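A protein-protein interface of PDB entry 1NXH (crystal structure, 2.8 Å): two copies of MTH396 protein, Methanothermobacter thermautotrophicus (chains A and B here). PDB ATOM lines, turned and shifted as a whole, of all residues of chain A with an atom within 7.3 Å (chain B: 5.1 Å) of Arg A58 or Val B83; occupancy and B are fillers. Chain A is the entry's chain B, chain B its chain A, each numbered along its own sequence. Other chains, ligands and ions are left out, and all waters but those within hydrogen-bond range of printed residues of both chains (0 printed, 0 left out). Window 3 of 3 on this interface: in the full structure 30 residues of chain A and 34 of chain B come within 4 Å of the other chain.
Of the printed residues of chain B, Leu A47 touches Met B84 (3.7 Å). Of chain B, only Val B83 (2.4 Å) and Glu B85 (3.2 Å) come within 4 Å of Arg A58. Printed residues of chain B within 4 Å of Arg A63: Trp B79. Printed residues of chain B within 4 Å of Cys A66: Cys B78 and Trp B79. Of the printed residues of chain A, Cys B78 touches Cys A66. Of chain A, only Arg A58 and Phe A59 come within 4 Å of Val B83. Of the printed residues of chain A, Met B84 touches Leu A47 and Phe A59.
Among the printed residues, pairs that only touch across the chains: Phe A59 with Met B84, Phe A59 with Val B83, Phe A59 with Trp B79, Leu A47 with Met B84 and Arg A63 with Trp B79.
Hydrophobic or aromatic side chains of chain A that line the printed part of chain B: Leu A47 and Phe A59. Hydrophobic or aromatic side chains of chain B that line the printed part of chain A: Trp B79, Val B83 and Met B84. Along chain B the printed residues that touch a printed residue of chain A span positions 78 to 85. Among the printed residues, Asp or Glu carboxylates within 4 Å of a Lys or Arg side-chain nitrogen of the other chain: Arg A58 with Glu B85 (3.2 Å).
No position is printed for both chains. Of the 9 pairs that touch across the chains among the printed residues, none has its exchanged pair printed and touching as well.
SG of Cys A66 is disulfide-bonded to SG of Cys B78, at 2.0 Å. The side-chain sulfur (SG) of Cys A66 sits close to the indole nitrogen (NE1) of Trp B79 (3.7 Å). The guanidinium group of Arg A58 lies within hydrogen-bond range of the backbone carbonyl oxygen of Val B83, 2.4 Å away. OE2 of Glu B85 lies within salt-bridge range of NH1 of Arg A58, at 3.2 Å.
O of Cys B78 lies within hydrogen-bond range of N of Val B83 (3.0 Å). The backbone carbonyl oxygen of Trp B79 lies within hydrogen-bond range of the backbone NH of Met B84, at 2.7 Å. O of Arg A58 lies within hydrogen-bond range of OG of Ser A61.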
ATOM      1  N   LEU A  47      14.909   0.950  28.888  1.00  0.00           N
ATOM      2  CA  LEU A  47      15.910  -0.092  29.074  1.00  0.00           C
ATOM      3  C   LEU A  47      15.960  -0.707  30.462  1.00  0.00           C
ATOM      4  O   LEU A  47      15.820  -0.016  31.467  1.00  0.00           O
ATOM      5  CB  LEU A  47      17.280   0.456  28.690  1.00  0.00           C
ATOM      6  CG  LEU A  47      17.377   0.624  27.173  1.00  0.00           C
ATOM      7  CD1 LEU A  47      18.009   1.958  26.817  1.00  0.00           C
ATOM      8  CD2 LEU A  47      18.153  -0.550  26.597  1.00  0.00           C
ATOM      9  N   ALA A  54      25.729  -2.955  29.681  1.00  0.00           N
ATOM     10  CA  ALA A  54      26.105  -3.652  28.453  1.00  0.00           C
ATOM     11  C   ALA A  54      26.109  -2.712  27.245  1.00  0.00           C
ATOM     12  O   ALA A  54      26.791  -2.959  26.252  1.00  0.00           O
ATOM     13  CB  ALA A  54      25.142  -4.818  28.202  1.00  0.00           C
ATOM     14  N   LEU A  55      25.361  -1.622  27.343  1.00  0.00           N
ATOM     15  CA  LEU A  55      25.261  -0.675  26.245  1.00  0.00           C
ATOM     16  C   LEU A  55      26.514   0.141  25.894  1.00  0.00           C
ATOM     17  O   LEU A  55      26.964   0.091  24.750  1.00  0.00           O
ATOM     18  CB  LEU A  55      24.064   0.265  26.480  1.00  0.00           C
ATOM     19  CG  LEU A  55      22.647  -0.355  26.420  1.00  0.00           C
ATOM     20  CD1 LEU A  55      21.595   0.753  26.518  1.00  0.00           C
ATOM     21  CD2 LEU A  55      22.453  -1.149  25.129  1.00  0.00           C
ATOM     22  N   HIS A  56      27.082   0.872  26.854  1.00  0.00           N
ATOM     23  CA  HIS A  56      28.263   1.713  26.587  1.00  0.00           C
ATOM     24  C   HIS A  56      29.270   1.066  25.620  1.00  0.00           C
ATOM     25  O   HIS A  56      29.590   1.638  24.576  1.00  0.00           O
ATOM     26  CB  HIS A  56      28.976   2.094  27.907  1.00  0.00           C
ATOM     27  CG  HIS A  56      29.463   3.518  27.966  1.00  0.00           C
ATOM     28  ND1 HIS A  56      28.658   4.569  28.358  1.00  0.00           N
ATOM     29  CD2 HIS A  56      30.679   4.060  27.702  1.00  0.00           C
ATOM     30  CE1 HIS A  56      29.354   5.691  28.334  1.00  0.00           C
ATOM     31  NE2 HIS A  56      30.583   5.412  27.939  1.00  0.00           N
ATOM     32  N   PRO A  57      29.764  -0.143  25.942  1.00  0.00           N
ATOM     33  CA  PRO A  57      30.735  -0.823  25.074  1.00  0.00           C
ATOM     34  C   PRO A  57      30.225  -0.912  23.650  1.00  0.00           C
ATOM     35  O   PRO A  57      30.851  -0.431  22.706  1.00  0.00           O
ATOM     36  CB  PRO A  57      30.860  -2.207  25.702  1.00  0.00           C
ATOM     37  CG  PRO A  57      30.444  -1.990  27.130  1.00  0.00           C
ATOM     38  CD  PRO A  57      29.285  -1.056  26.992  1.00  0.00           C
ATOM     39  N   ARG A  58      29.073  -1.552  23.516  1.00  0.00           N
ATOM     40  CA  ARG A  58      28.430  -1.725  22.228  1.00  0.00           C
ATOM     41  C   ARG A  58      28.262  -0.350  21.594  1.00  0.00           C
ATOM     42  O   ARG A  58      28.297  -0.222  20.374  1.00  0.00           O
ATOM     43  CB  ARG A  58      27.062  -2.379  22.419  1.00  0.00           C
ATOM     44  CG  ARG A  58      26.389  -2.812  21.142  1.00  0.00           C
ATOM     45  CD  ARG A  58      24.881  -2.793  21.334  1.00  0.00           C
ATOM     46  NE  ARG A  58      24.273  -4.123  21.451  1.00  0.00           N
ATOM     47  CZ  ARG A  58      22.954  -4.349  21.505  1.00  0.00           C
ATOM     48  NH1 ARG A  58      22.092  -3.338  21.456  1.00  0.00           N
ATOM     49  NH2 ARG A  58      22.485  -5.590  21.590  1.00  0.00           N
ATOM     50  N   PHE A  59      28.079   0.667  22.438  1.00  0.00           N
ATOM     51  CA  PHE A  59      27.906   2.047  21.987  1.00  0.00           C
ATOM     52  C   PHE A  59      29.158   2.574  21.319  1.00  0.00           C
ATOM     53  O   PHE A  59      29.107   3.140  20.230  1.00  0.00           O
ATOM     54  CB  PHE A  59      27.596   2.983  23.160  1.00  0.00           C
ATOM     55  CG  PHE A  59      26.183   2.931  23.641  1.00  0.00           C
ATOM     56  CD1 PHE A  59      25.763   3.786  24.654  1.00  0.00           C
ATOM     57  CD2 PHE A  59      25.265   2.049  23.084  1.00  0.00           C
ATOM     58  CE1 PHE A  59      24.449   3.770  25.109  1.00  0.00           C
ATOM     59  CE2 PHE A  59      23.945   2.021  23.529  1.00  0.00           C
ATOM     60  CZ  PHE A  59      23.536   2.885  24.545  1.00  0.00           C
ATOM     61  N   GLU A  60      30.286   2.404  21.992  1.00  0.00           N
ATOM     62  CA  GLU A  60      31.552   2.892  21.479  1.00  0.00           C
ATOM     63  C   GLU A  60      31.965   2.205  20.184  1.00  0.00           C
ATOM     64  O   GLU A  60      32.602   2.821  19.330  1.00  0.00           O
ATOM     65  CB  GLU A  60      32.633   2.723  22.547  1.00  0.00           C
ATOM     66  CG  GLU A  60      32.270   3.370  23.888  1.00  0.00           C
ATOM     67  CD  GLU A  60      32.324   4.890  23.863  1.00  0.00           C
ATOM     68  OE1 GLU A  60      32.078   5.484  22.791  1.00  0.00           O
ATOM     69  OE2 GLU A  60      32.601   5.493  24.925  1.00  0.00           O
ATOM     70  N   SER A  61      31.590   0.938  20.030  1.00  0.00           N
ATOM     71  CA  SER A  61      31.931   0.168  18.830  1.00  0.00           C
ATOM     72  C   SER A  61      31.031   0.479  17.628  1.00  0.00           C
ATOM     73  O   SER A  61      31.245  -0.042  16.535  1.00  0.00           O
ATOM     74  CB  SER A  61      31.868  -1.335  19.129  1.00  0.00           C
ATOM     75  OG  SER A  61      30.549  -1.748  19.464  1.00  0.00           O
ATOM     76  N   ALA A  62      30.026   1.328  17.832  1.00  0.00           N
ATOM     77  CA  ALA A  62      29.099   1.693  16.764  1.00  0.00           C
ATOM     78  C   ALA A  62      29.052   3.206  16.538  1.00  0.00           C
ATOM     79  O   ALA A  62      28.418   3.677  15.589  1.00  0.00           O
ATOM     80  CB  ALA A  62      27.697   1.165  17.087  1.00  0.00           C
ATOM     81  N   ARG A  63      29.717   3.965  17.405  1.00  0.00           N
ATOM     82  CA  ARG A  63      29.752   5.422  17.272  1.00  0.00           C
ATOM     83  C   ARG A  63      30.270   5.816  15.877  1.00  0.00           C
ATOM     84  O   ARG A  63      29.774   6.771  15.280  1.00  0.00           O
ATOM     85  CB  ARG A  63      30.606   6.035  18.388  1.00  0.00           C
ATOM     86  CG  ARG A  63      30.425   7.543  18.539  1.00  0.00           C
ATOM     87  CD  ARG A  63      30.505   7.996  20.002  1.00  0.00           C
ATOM     88  NE  ARG A  63      31.100   9.327  20.153  1.00  0.00           N
ATOM     89  CZ  ARG A  63      32.414   9.574  20.165  1.00  0.00           C
ATOM     90  NH1 ARG A  63      33.296   8.581  20.043  1.00  0.00           N
ATOM     91  NH2 ARG A  63      32.854  10.823  20.286  1.00  0.00           N
ATOM     92  N   PRO A  64      31.277   5.087  15.339  1.00  0.00           N
ATOM     93  CA  PRO A  64      31.824   5.379  14.006  1.00  0.00           C
ATOM     94  C   PRO A  64      30.752   5.151  12.968  1.00  0.00           C
ATOM     95  O   PRO A  64      30.384   6.060  12.223  1.00  0.00           O
ATOM     96  CB  PRO A  64      32.934   4.357  13.850  1.00  0.00           C
ATOM     97  CG  PRO A  64      33.435   4.223  15.234  1.00  0.00           C
ATOM     98  CD  PRO A  64      32.158   4.139  16.049  1.00  0.00           C
ATOM     99  N   ARG A  65      30.260   3.918  12.929  1.00  0.00           N
ATOM    100  CA  ARG A  65      29.213   3.524  11.993  1.00  0.00           C
ATOM    101  C   ARG A  65      28.081   4.550  11.936  1.00  0.00           C
ATOM    102  O   ARG A  65      27.694   5.014  10.859  1.00  0.00           O
ATOM    103  CB  ARG A  65      28.651   2.169  12.405  1.00  0.00           C
ATOM    104  CG  ARG A  65      27.353   1.779  11.727  1.00  0.00           C
ATOM    105  CD  ARG A  65      26.738   0.647  12.513  1.00  0.00           C
ATOM    106  NE  ARG A  65      27.775  -0.305  12.906  1.00  0.00           N
ATOM    107  CZ  ARG A  65      28.430  -1.097  12.056  1.00  0.00           C
ATOM    108  NH1 ARG A  65      28.152  -1.061  10.752  1.00  0.00           N
ATOM    109  NH2 ARG A  65      29.378  -1.916  12.508  1.00  0.00           N
ATOM    110  N   CYS A  66      27.559   4.910  13.104  1.00  0.00           N
ATOM    111  CA  CYS A  66      26.463   5.861  13.180  1.00  0.00           C
ATOM    112  C   CYS A  66      26.809   7.218  12.622  1.00  0.00           C
ATOM    113  O   CYS A  66      25.951   7.930  12.114  1.00  0.00           O
ATOM    114  CB  CYS A  66      25.993   6.029  14.616  1.00  0.00           C
ATOM    115  SG  CYS A  66      25.001   4.649  15.251  1.00  0.00           S
ATOM    116  N   CYS B  78      19.849   5.380  14.292  1.00  0.00           N
ATOM    117  CA  CYS B  78      20.975   4.450  14.305  1.00  0.00           C
ATOM    118  C   CYS B  78      21.106   4.014  15.758  1.00  0.00           C
ATOM    119  O   CYS B  78      21.330   2.842  16.055  1.00  0.00           O
ATOM    120  CB  CYS B  78      22.269   5.153  13.867  1.00  0.00           C
ATOM    121  SG  CYS B  78      23.769   4.110  13.713  1.00  0.00           S
ATOM    122  N   TRP B  79      20.934   4.984  16.655  1.00  0.00           N
ATOM    123  CA  TRP B  79      21.058   4.761  18.086  1.00  0.00           C
ATOM    124  C   TRP B  79      19.802   4.221  18.712  1.00  0.00           C
ATOM    125  O   TRP B  79      19.801   3.149  19.327  1.00  0.00           O
ATOM    126  CB  TRP B  79      21.425   6.064  18.788  1.00  0.00           C
ATOM    127  CG  TRP B  79      22.777   6.539  18.453  1.00  0.00           C
ATOM    128  CD1 TRP B  79      23.116   7.465  17.511  1.00  0.00           C
ATOM    129  CD2 TRP B  79      23.999   6.073  19.023  1.00  0.00           C
ATOM    130  NE1 TRP B  79      24.488   7.606  17.455  1.00  0.00           N
ATOM    131  CE2 TRP B  79      25.053   6.761  18.375  1.00  0.00           C
ATOM    132  CE3 TRP B  79      24.309   5.139  20.021  1.00  0.00           C
ATOM    133  CZ2 TRP B  79      26.392   6.543  18.691  1.00  0.00           C
ATOM    134  CZ3 TRP B  79      25.639   4.922  20.339  1.00  0.00           C
ATOM    135  CH2 TRP B  79      26.668   5.623  19.674  1.00  0.00           C
ATOM    136  N   VAL B  81      17.475   2.680  17.628  1.00  0.00           N
ATOM    137  CA  VAL B  81      17.064   1.356  17.233  1.00  0.00           C
ATOM    138  C   VAL B  81      18.218   0.383  17.091  1.00  0.00           C
ATOM    139  O   VAL B  81      18.450  -0.459  17.972  1.00  0.00           O
ATOM    140  CB  VAL B  81      16.268   1.444  15.937  1.00  0.00           C
ATOM    141  CG1 VAL B  81      15.811   0.068  15.486  1.00  0.00           C
ATOM    142  CG2 VAL B  81      15.058   2.363  16.162  1.00  0.00           C
ATOM    143  N   ASP B  82      18.963   0.508  16.003  1.00  0.00           N
ATOM    144  CA  ASP B  82      20.072  -0.397  15.742  1.00  0.00           C
ATOM    145  C   ASP B  82      20.973  -0.656  16.951  1.00  0.00           C
ATOM    146  O   ASP B  82      21.426  -1.784  17.167  1.00  0.00           O
ATOM    147  CB  ASP B  82      20.913   0.143  14.582  1.00  0.00           C
ATOM    148  CG  ASP B  82      20.059   0.628  13.398  1.00  0.00           C
ATOM    149  OD1 ASP B  82      20.645   0.959  12.339  1.00  0.00           O
ATOM    150  OD2 ASP B  82      18.811   0.693  13.517  1.00  0.00           O
ATOM    151  N   VAL B  83      21.222   0.373  17.753  1.00  0.00           N
ATOM    152  CA  VAL B  83      22.108   0.231  18.906  1.00  0.00           C
ATOM    153  C   VAL B  83      21.447  -0.006  20.252  1.00  0.00           C
ATOM    154  O   VAL B  83      21.609  -1.058  20.850  1.00  0.00           O
ATOM    155  CB  VAL B  83      22.995   1.464  19.071  1.00  0.00           C
ATOM    156  CG1 VAL B  83      23.964   1.238  20.192  1.00  0.00           C
ATOM    157  CG2 VAL B  83      23.724   1.753  17.797  1.00  0.00           C
ATOM    158  N   MET B  84      20.725   0.992  20.742  1.00  0.00           N
ATOM    159  CA  MET B  84      20.079   0.872  22.035  1.00  0.00           C
ATOM    160  C   MET B  84      18.809   0.021  21.997  1.00  0.00           C
ATOM    161  O   MET B  84      18.520  -0.717  22.938  1.00  0.00           O
ATOM    162  CB  MET B  84      19.795   2.271  22.599  1.00  0.00           C
ATOM    163  CG  MET B  84      21.025   3.168  22.570  1.00  0.00           C
ATOM    164  SD  MET B  84      20.874   4.835  23.533  1.00  0.00           S
ATOM    165  CE  MET B  84      20.267   5.989  22.148  1.00  0.00           C
ATOM    166  N   GLU B  85      18.057   0.097  20.909  1.00  0.00           N
ATOM    167  CA  GLU B  85      16.825  -0.678  20.808  1.00  0.00           C
ATOM    168  C   GLU B  85      15.721  -0.105  21.699  1.00  0.00           C
ATOM    169  O   GLU B  85      14.843  -0.822  22.158  1.00  0.00           O
ATOM    170  CB  GLU B  85      17.079  -2.139  21.178  1.00  0.00           C
ATOM    171  CG  GLU B  85      18.134  -2.813  20.344  1.00  0.00           C
ATOM    172  CD  GLU B  85      18.215  -4.294  20.645  1.00  0.00           C
ATOM    173  OE1 GLU B  85      17.177  -4.976  20.514  1.00  0.00           O
ATOM    174  OE2 GLU B  85      19.304  -4.781  21.020  1.00  0.00           O
